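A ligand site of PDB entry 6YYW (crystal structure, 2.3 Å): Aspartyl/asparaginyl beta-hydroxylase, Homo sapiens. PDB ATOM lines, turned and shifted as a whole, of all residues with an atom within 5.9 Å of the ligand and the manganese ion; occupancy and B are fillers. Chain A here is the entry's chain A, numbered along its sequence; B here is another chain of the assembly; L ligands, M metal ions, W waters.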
ATOM      1  N   LEU A 290      -9.518  31.279 -18.325  1.00  0.00           N
ATOM      2  CA  LEU A 290      -9.801  31.175 -19.756  1.00  0.00           C
ATOM      3  C   LEU A 290     -11.272  31.376 -20.131  1.00  0.00           C
ATOM      4  O   LEU A 290     -11.569  31.376 -21.340  1.00  0.00           O
ATOM      5  CB  LEU A 290      -9.346  29.798 -20.299  1.00  0.00           C
ATOM      6  CG  LEU A 290      -7.852  29.541 -20.113  1.00  0.00           C
ATOM      7  CD1 LEU A 290      -7.381  28.201 -20.641  1.00  0.00           C
ATOM      8  CD2 LEU A 290      -7.068  30.660 -20.756  1.00  0.00           C
ATOM      9  N   TRP A 296     -17.365  25.246 -16.931  1.00  0.00           N
ATOM     10  CA  TRP A 296     -16.413  24.404 -17.652  1.00  0.00           C
ATOM     11  C   TRP A 296     -15.526  23.727 -16.611  1.00  0.00           C
ATOM     12  O   TRP A 296     -14.898  24.404 -15.796  1.00  0.00           O
ATOM     13  CB  TRP A 296     -15.586  25.248 -18.629  1.00  0.00           C
ATOM     14  CG  TRP A 296     -14.459  24.525 -19.339  1.00  0.00           C
ATOM     15  CD1 TRP A 296     -14.361  23.202 -19.586  1.00  0.00           C
ATOM     16  CD2 TRP A 296     -13.301  25.133 -19.953  1.00  0.00           C
ATOM     17  NE1 TRP A 296     -13.218  22.934 -20.283  1.00  0.00           N
ATOM     18  CE2 TRP A 296     -12.535  24.092 -20.515  1.00  0.00           C
ATOM     19  CE3 TRP A 296     -12.822  26.435 -20.026  1.00  0.00           C
ATOM     20  CZ2 TRP A 296     -11.307  24.320 -21.151  1.00  0.00           C
ATOM     21  CZ3 TRP A 296     -11.620  26.667 -20.688  1.00  0.00           C
ATOM     22  CH2 TRP A 296     -10.875  25.625 -21.244  1.00  0.00           C
ATOM     23  N   GLN A 298     -13.060  19.919 -15.520  1.00  0.00           N
ATOM     24  CA  GLN A 298     -12.258  18.849 -16.108  1.00  0.00           C
ATOM     25  C   GLN A 298     -11.859  17.854 -15.032  1.00  0.00           C
ATOM     26  O   GLN A 298     -11.568  18.215 -13.900  1.00  0.00           O
ATOM     27  CB  GLN A 298     -11.031  19.361 -16.839  1.00  0.00           C
ATOM     28  CG  GLN A 298     -11.420  20.475 -17.738  1.00  0.00           C
ATOM     29  CD  GLN A 298     -10.247  21.004 -18.456  1.00  0.00           C
ATOM     30  OE1 GLN A 298     -10.080  20.756 -19.651  1.00  0.00           O
ATOM     31  NE2 GLN A 298      -9.422  21.775 -17.754  1.00  0.00           N
ATOM     32  N   SER A 339     -13.631  16.539 -20.121  1.00  0.00           N
ATOM     33  CA  SER A 339     -13.909  17.963 -20.119  1.00  0.00           C
ATOM     34  C   SER A 339     -15.402  18.171 -20.308  1.00  0.00           C
ATOM     35  O   SER A 339     -15.944  17.798 -21.374  1.00  0.00           O
ATOM     36  CB  SER A 339     -13.092  18.598 -21.238  1.00  0.00           C
ATOM     37  OG  SER A 339     -13.397  19.960 -21.319  1.00  0.00           O
ATOM     38  N   ILE A 340     -16.075  18.785 -19.333  1.00  0.00           N
ATOM     39  CA  ILE A 340     -17.515  19.051 -19.414  1.00  0.00           C
ATOM     40  C   ILE A 340     -17.748  20.555 -19.557  1.00  0.00           C
ATOM     41  O   ILE A 340     -17.118  21.375 -18.878  1.00  0.00           O
ATOM     42  CB  ILE A 340     -18.296  18.457 -18.214  1.00  0.00           C
ATOM     43  CG1 ILE A 340     -19.763  18.386 -18.628  1.00  0.00           C
ATOM     44  CG2 ILE A 340     -18.023  19.174 -16.830  1.00  0.00           C
ATOM     45  CD1 ILE A 340     -20.715  17.677 -17.672  1.00  0.00           C
ATOM     46  N   MET A 341     -18.660  20.936 -20.468  1.00  0.00           N
ATOM     47  CA  MET A 341     -18.970  22.344 -20.698  1.00  0.00           C
ATOM     48  C   MET A 341     -20.477  22.497 -20.854  1.00  0.00           C
ATOM     49  O   MET A 341     -21.081  21.710 -21.582  1.00  0.00           O
ATOM     50  CB  MET A 341     -18.248  22.876 -21.948  1.00  0.00           C
ATOM     51  CG  MET A 341     -18.111  24.405 -22.047  1.00  0.00           C
ATOM     52  SD  MET A 341     -17.135  24.870 -23.476  1.00  0.00           S
ATOM     53  CE  MET A 341     -15.487  24.190 -23.091  1.00  0.00           C
ATOM     54  N   VAL A 347     -15.339  30.317 -24.134  1.00  0.00           N
ATOM     55  CA  VAL A 347     -13.917  30.275 -23.778  1.00  0.00           C
ATOM     56  C   VAL A 347     -13.199  31.339 -24.583  1.00  0.00           C
ATOM     57  O   VAL A 347     -13.207  31.322 -25.804  1.00  0.00           O
ATOM     58  CB  VAL A 347     -13.306  28.892 -24.043  1.00  0.00           C
ATOM     59  CG1 VAL A 347     -11.751  28.896 -23.736  1.00  0.00           C
ATOM     60  CG2 VAL A 347     -13.988  27.824 -23.227  1.00  0.00           C
ATOM     61  N   HIS A 350      -7.269  31.742 -26.841  1.00  0.00           N
ATOM     62  CA  HIS A 350      -6.088  31.447 -26.034  1.00  0.00           C
ATOM     63  C   HIS A 350      -5.224  30.425 -26.766  1.00  0.00           C
ATOM     64  O   HIS A 350      -5.632  29.837 -27.762  1.00  0.00           O
ATOM     65  CB  HIS A 350      -6.482  30.918 -24.645  1.00  0.00           C
ATOM     66  CG  HIS A 350      -7.062  29.526 -24.648  1.00  0.00           C
ATOM     67  ND1 HIS A 350      -8.383  29.261 -24.938  1.00  0.00           N
ATOM     68  CD2 HIS A 350      -6.501  28.331 -24.355  1.00  0.00           C
ATOM     69  CE1 HIS A 350      -8.608  27.968 -24.864  1.00  0.00           C
ATOM     70  NE2 HIS A 350      -7.486  27.373 -24.490  1.00  0.00           N
ATOM     71  N   GLY A 352      -2.059  27.342 -26.046  1.00  0.00           N
ATOM     72  CA  GLY A 352      -1.344  26.512 -25.116  1.00  0.00           C
ATOM     73  C   GLY A 352       0.103  26.939 -24.976  1.00  0.00           C
ATOM     74  O   GLY A 352       0.619  27.786 -25.720  1.00  0.00           O
ATOM     75  N   ARG A 357       3.034  19.288 -28.391  1.00  0.00           N
ATOM     76  CA  ARG A 357       1.906  18.381 -28.259  1.00  0.00           C
ATOM     77  C   ARG A 357       0.838  18.709 -29.303  1.00  0.00           C
ATOM     78  O   ARG A 357       0.774  19.821 -29.843  1.00  0.00           O
ATOM     79  CB  ARG A 357       1.330  18.431 -26.839  1.00  0.00           C
ATOM     80  CG  ARG A 357       0.550  19.684 -26.546  1.00  0.00           C
ATOM     81  CD  ARG A 357      -0.240  19.575 -25.240  1.00  0.00           C
ATOM     82  NE  ARG A 357      -1.069  20.746 -25.035  1.00  0.00           N
ATOM     83  CZ  ARG A 357      -1.083  21.483 -23.931  1.00  0.00           C
ATOM     84  NH1 ARG A 357      -0.358  21.145 -22.873  1.00  0.00           N
ATOM     85  NH2 ARG A 357      -1.876  22.533 -23.869  1.00  0.00           N
ATOM     86  N   ARG A 359      -3.430  17.792 -29.612  1.00  0.00           N
ATOM     87  CA  ARG A 359      -4.562  17.542 -28.736  1.00  0.00           C
ATOM     88  C   ARG A 359      -5.674  16.848 -29.511  1.00  0.00           C
ATOM     89  O   ARG A 359      -6.116  17.311 -30.586  1.00  0.00           O
ATOM     90  CB  ARG A 359      -5.030  18.860 -28.115  1.00  0.00           C
ATOM     91  CG  ARG A 359      -6.111  18.849 -27.034  1.00  0.00           C
ATOM     92  CD  ARG A 359      -5.914  20.086 -26.172  1.00  0.00           C
ATOM     93  NE  ARG A 359      -5.051  19.767 -25.040  1.00  0.00           N
ATOM     94  CZ  ARG A 359      -4.992  20.473 -23.914  1.00  0.00           C
ATOM     95  NH1 ARG A 359      -5.758  21.561 -23.771  1.00  0.00           N
ATOM     96  NH2 ARG A 359      -4.169  20.116 -22.931  1.00  0.00           N
ATOM     97  N   HIS A 361      -9.570  15.335 -29.356  1.00  0.00           N
ATOM     98  CA  HIS A 361     -10.871  15.361 -28.705  1.00  0.00           C
ATOM     99  C   HIS A 361     -11.735  14.215 -29.207  1.00  0.00           C
ATOM    100  O   HIS A 361     -11.984  14.119 -30.411  1.00  0.00           O
ATOM    101  CB  HIS A 361     -11.643  16.637 -29.022  1.00  0.00           C
ATOM    102  CG  HIS A 361     -11.157  17.850 -28.338  1.00  0.00           C
ATOM    103  ND1 HIS A 361     -11.809  19.054 -28.459  1.00  0.00           N
ATOM    104  CD2 HIS A 361     -10.120  18.057 -27.493  1.00  0.00           C
ATOM    105  CE1 HIS A 361     -11.187  19.960 -27.720  1.00  0.00           C
ATOM    106  NE2 HIS A 361     -10.167  19.375 -27.124  1.00  0.00           N
ATOM    107  N   ILE A 373     -15.968  24.813 -31.996  1.00  0.00           N
ATOM    108  CA  ILE A 373     -14.591  25.145 -31.629  1.00  0.00           C
ATOM    109  C   ILE A 373     -13.856  25.673 -32.862  1.00  0.00           C
ATOM    110  O   ILE A 373     -13.799  25.008 -33.906  1.00  0.00           O
ATOM    111  CB  ILE A 373     -13.845  23.932 -31.038  1.00  0.00           C
ATOM    112  CG1 ILE A 373     -12.388  24.218 -30.718  1.00  0.00           C
ATOM    113  CG2 ILE A 373     -13.778  22.747 -31.997  1.00  0.00           C
ATOM    114  CD1 ILE A 373     -11.537  23.011 -30.272  1.00  0.00           C
ATOM    115  N   TRP A 382     -17.842  18.854 -32.882  1.00  0.00           N
ATOM    116  CA  TRP A 382     -17.607  17.493 -32.407  1.00  0.00           C
ATOM    117  C   TRP A 382     -18.699  16.550 -32.934  1.00  0.00           C
ATOM    118  O   TRP A 382     -19.813  16.958 -33.257  1.00  0.00           O
ATOM    119  CB  TRP A 382     -17.598  17.437 -30.863  1.00  0.00           C
ATOM    120  CG  TRP A 382     -16.500  18.284 -30.248  1.00  0.00           C
ATOM    121  CD1 TRP A 382     -15.205  17.913 -30.039  1.00  0.00           C
ATOM    122  CD2 TRP A 382     -16.614  19.648 -29.823  1.00  0.00           C
ATOM    123  NE1 TRP A 382     -14.491  18.980 -29.511  1.00  0.00           N
ATOM    124  CE2 TRP A 382     -15.347  20.046 -29.365  1.00  0.00           C
ATOM    125  CE3 TRP A 382     -17.665  20.563 -29.769  1.00  0.00           C
ATOM    126  CZ2 TRP A 382     -15.114  21.328 -28.851  1.00  0.00           C
ATOM    127  CZ3 TRP A 382     -17.434  21.826 -29.288  1.00  0.00           C
ATOM    128  CH2 TRP A 382     -16.167  22.203 -28.818  1.00  0.00           C
ATOM    129  N   PHE A 390      -6.223  18.896 -33.199  1.00  0.00           N
ATOM    130  CA  PHE A 390      -5.812  20.254 -33.503  1.00  0.00           C
ATOM    131  C   PHE A 390      -4.549  20.568 -32.691  1.00  0.00           C
ATOM    132  O   PHE A 390      -4.170  19.825 -31.769  1.00  0.00           O
ATOM    133  CB  PHE A 390      -6.983  21.238 -33.272  1.00  0.00           C
ATOM    134  CG  PHE A 390      -7.281  21.490 -31.850  1.00  0.00           C
ATOM    135  CD1 PHE A 390      -8.075  20.594 -31.121  1.00  0.00           C
ATOM    136  CD2 PHE A 390      -6.730  22.574 -31.196  1.00  0.00           C
ATOM    137  CE1 PHE A 390      -8.320  20.781 -29.795  1.00  0.00           C
ATOM    138  CE2 PHE A 390      -6.954  22.766 -29.862  1.00  0.00           C
ATOM    139  CZ  PHE A 390      -7.749  21.871 -29.155  1.00  0.00           C
ATOM    140  N   ASP A 392      -3.189  22.945 -30.203  1.00  0.00           N
ATOM    141  CA  ASP A 392      -3.647  23.992 -29.307  1.00  0.00           C
ATOM    142  C   ASP A 392      -2.556  25.009 -29.067  1.00  0.00           C
ATOM    143  O   ASP A 392      -2.840  25.993 -28.396  1.00  0.00           O
ATOM    144  CB  ASP A 392      -4.210  23.394 -27.998  1.00  0.00           C
ATOM    145  CG  ASP A 392      -3.182  23.236 -26.888  1.00  0.00           C
ATOM    146  OD1 ASP A 392      -2.083  22.721 -27.153  1.00  0.00           O
ATOM    147  OD2 ASP A 392      -3.492  23.631 -25.726  1.00  0.00           O
ATOM    148  N   HIS A 396      -7.122  29.390 -30.153  1.00  0.00           N
ATOM    149  CA  HIS A 396      -8.360  28.663 -30.314  1.00  0.00           C
ATOM    150  C   HIS A 396      -9.412  29.139 -29.336  1.00  0.00           C
ATOM    151  O   HIS A 396      -9.122  29.761 -28.322  1.00  0.00           O
ATOM    152  CB  HIS A 396      -8.105  27.158 -30.212  1.00  0.00           C
ATOM    153  CG  HIS A 396      -7.541  26.707 -28.910  1.00  0.00           C
ATOM    154  ND1 HIS A 396      -6.203  26.783 -28.619  1.00  0.00           N
ATOM    155  CD2 HIS A 396      -8.117  26.124 -27.847  1.00  0.00           C
ATOM    156  CE1 HIS A 396      -5.973  26.277 -27.424  1.00  0.00           C
ATOM    157  NE2 HIS A 396      -7.123  25.869 -26.929  1.00  0.00           N
ATOM    158  N   VAL A 398     -13.892  28.576 -28.135  1.00  0.00           N
ATOM    159  CA  VAL A 398     -14.964  27.604 -27.983  1.00  0.00           C
ATOM    160  C   VAL A 398     -16.195  28.279 -27.432  1.00  0.00           C
ATOM    161  O   VAL A 398     -16.110  29.206 -26.618  1.00  0.00           O
ATOM    162  CB  VAL A 398     -14.489  26.451 -27.060  1.00  0.00           C
ATOM    163  CG1 VAL A 398     -15.613  25.616 -26.646  1.00  0.00           C
ATOM    164  CG2 VAL A 398     -13.401  25.608 -27.775  1.00  0.00           C
ATOM    165  N   ARG A 406     -22.386  19.206 -22.578  1.00  0.00           N
ATOM    166  CA  ARG A 406     -21.508  18.693 -23.630  1.00  0.00           C
ATOM    167  C   ARG A 406     -20.230  18.131 -23.015  1.00  0.00           C
ATOM    168  O   ARG A 406     -19.522  18.846 -22.297  1.00  0.00           O
ATOM    169  CB  ARG A 406     -21.091  19.787 -24.623  1.00  0.00           C
ATOM    170  CG  ARG A 406     -20.247  19.269 -25.808  1.00  0.00           C
ATOM    171  CD  ARG A 406     -18.989  20.073 -26.021  1.00  0.00           C
ATOM    172  NE  ARG A 406     -18.159  19.864 -24.844  1.00  0.00           N
ATOM    173  CZ  ARG A 406     -16.929  20.367 -24.647  1.00  0.00           C
ATOM    174  NH1 ARG A 406     -16.358  21.165 -25.550  1.00  0.00           N
ATOM    175  NH2 ARG A 406     -16.240  20.126 -23.528  1.00  0.00           N
ATOM    176  N   ILE A 408     -16.652  15.739 -23.640  1.00  0.00           N
ATOM    177  CA  ILE A 408     -15.660  15.249 -24.585  1.00  0.00           C
ATOM    178  C   ILE A 408     -14.539  14.654 -23.744  1.00  0.00           C
ATOM    179  O   ILE A 408     -14.415  14.929 -22.549  1.00  0.00           O
ATOM    180  CB  ILE A 408     -15.111  16.352 -25.531  1.00  0.00           C
ATOM    181  CG1 ILE A 408     -14.225  17.315 -24.722  1.00  0.00           C
ATOM    182  CG2 ILE A 408     -16.262  17.072 -26.367  1.00  0.00           C
ATOM    183  CD1 ILE A 408     -13.634  18.520 -25.498  1.00  0.00           C
ATOM    184  N   ILE A 410     -10.332  14.355 -23.765  1.00  0.00           N
ATOM    185  CA  ILE A 410      -9.158  15.066 -24.306  1.00  0.00           C
ATOM    186  C   ILE A 410      -7.896  14.235 -24.039  1.00  0.00           C
ATOM    187  O   ILE A 410      -7.599  13.882 -22.887  1.00  0.00           O
ATOM    188  CB  ILE A 410      -8.998  16.454 -23.657  1.00  0.00           C
ATOM    189  CG1 ILE A 410     -10.277  17.280 -23.794  1.00  0.00           C
ATOM    190  CG2 ILE A 410      -7.773  17.218 -24.220  1.00  0.00           C
ATOM    191  CD1 ILE A 410     -10.185  18.709 -23.255  1.00  0.00           C
ATOM    192  N   ASP B  18      -3.765  24.345 -19.911  1.00  0.00           N
ATOM    193  CA  ASP B  18      -4.345  24.873 -21.145  1.00  0.00           C
ATOM    194  C   ASP B  18      -3.800  26.225 -21.631  1.00  0.00           C
ATOM    195  O   ASP B  18      -4.004  26.571 -22.802  1.00  0.00           O
ATOM    196  CB  ASP B  18      -5.860  25.033 -20.968  1.00  0.00           C
ATOM    197  CG  ASP B  18      -6.631  23.917 -21.621  1.00  0.00           C
ATOM    198  OD1 ASP B  18      -6.554  22.762 -21.027  1.00  0.00           O
ATOM    199  OD2 ASP B  18      -7.224  24.258 -22.740  1.00  0.00           O
HETATM  200  C1  LIG L   1      -8.527  22.662 -25.417  1.00  0.00           C
HETATM  201  O1  LIG L   1      -8.986  21.528 -25.658  1.00  0.00           O
HETATM  202  O2  LIG L   1      -7.339  23.084 -25.461  1.00  0.00           O
HETATM  203  C2  LIG L   1      -9.624  23.532 -25.000  1.00  0.00           C
HETATM  204  O3  LIG L   1      -9.557  24.719 -25.013  1.00  0.00           O
HETATM  205  C3  LIG L   1     -10.744  22.505 -24.723  1.00  0.00           C
HETATM  206  C4  LIG L   1     -12.154  22.968 -24.475  1.00  0.00           C
HETATM  207  C5  LIG L   1     -13.386  22.132 -24.333  1.00  0.00           C
HETATM  208  O4  LIG L   1     -14.183  22.354 -25.233  1.00  0.00           O
HETATM  209  O5  LIG L   1     -13.566  21.361 -23.415  1.00  0.00           O
HETATM  210 MN    MN M   1      -7.364  25.199 -24.982  1.00  0.00          MN
HETATM  211  O   HOH W   1      -5.320  25.021 -24.529  1.00  0.00           O
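O of Val 398 sits at hydrogen-bond distance from N of Val 347 (2.8 Å).
The backbone NH (N) of Arg 359 lies within hydrogen-bond range of the backbone carbonyl oxygen (O) of Phe 390 (3.1 Å).
The backbone NH of Ser 339 lies within hydrogen-bond range of the backbone carbonyl oxygen of Ile 408 (3.0 Å).
OG of Ser 339 lies within hydrogen-bond range of NE1 of Trp 296.
O of Arg 406 sits at hydrogen-bond distance from N of Met 341 (2.9 Å).
The guanidinium group (NH1) of Arg 359 is in salt-bridge range of the side-chain carboxylate (OD1) of Asp 18 of chain B (3.1 Å).
The guanidinium group of Arg 359 lies within salt-bridge range of the side-chain carboxylate of Asp 392.
O of Ser 339 lies within hydrogen-bond range of NH2 of Arg 406 (3.2 Å).
NE2 of His 361 is in hydrogen-bond range of O1 of the ligand.
The guanidinium group (NH1) of Arg 406 lies within salt-bridge range of an oxygen (O4) of the ligand.
The side-chain hydroxyl (OG) of Ser 339 sits at hydrogen-bond distance from an oxygen (O5) of the ligand (2.5 Å).
The guanidinium group (NH1) of Arg 359 is in salt-bridge range of an oxygen (O1) of the ligand (3.7 Å).
Water W1 lies within hydrogen-bond range of OD2 of Asp 392 and O of Asp 18 of chain B.
NE2 of His 396 binds the manganese ion.
The manganese ion is bound by water W1.
The manganese ion is bound by an oxygen (O2) of the ligand (2.2 Å).
NE2 of His 350 is bound to the manganese ion.
The manganese ion is bound by O3 of the ligand (2.2 Å).
The side-chain carboxylate (OD2) of Asp 18 of chain B binds the manganese ion, 2.4 Å away.
Of the 22 residues printed, 3 come within 4 Å of the manganese ion.
Along chain A the residues within 4 Å of the manganese ion span positions 350 to 396.
The nearest printed residue that does not touch the manganese ion is Arg 359 (4.2 Å).
Trp 296 touches the ligand.
Met 341 touches the ligand (CE to O4, 3.1 Å).
Trp 382 touches the ligand (CZ2 to O4, 3.9 Å).
CZ of Phe 390 touches O1 of the ligand, at 3.7 Å.
OD2 of Asp 392 touches O2 of the ligand, 3.9 Å away.
Val 398 touches the ligand.
CD1 of Ile 408 touches O5 of the ligand, 3.5 Å away.
CD1 of Ile 410 touches O1 of the ligand, at 3.9 Å.
Along chain A the residues within 4 Å of the ligand span positions 296 to 410.
The nearest printed residue that does not touch the ligand is Val 347 (4.9 Å).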
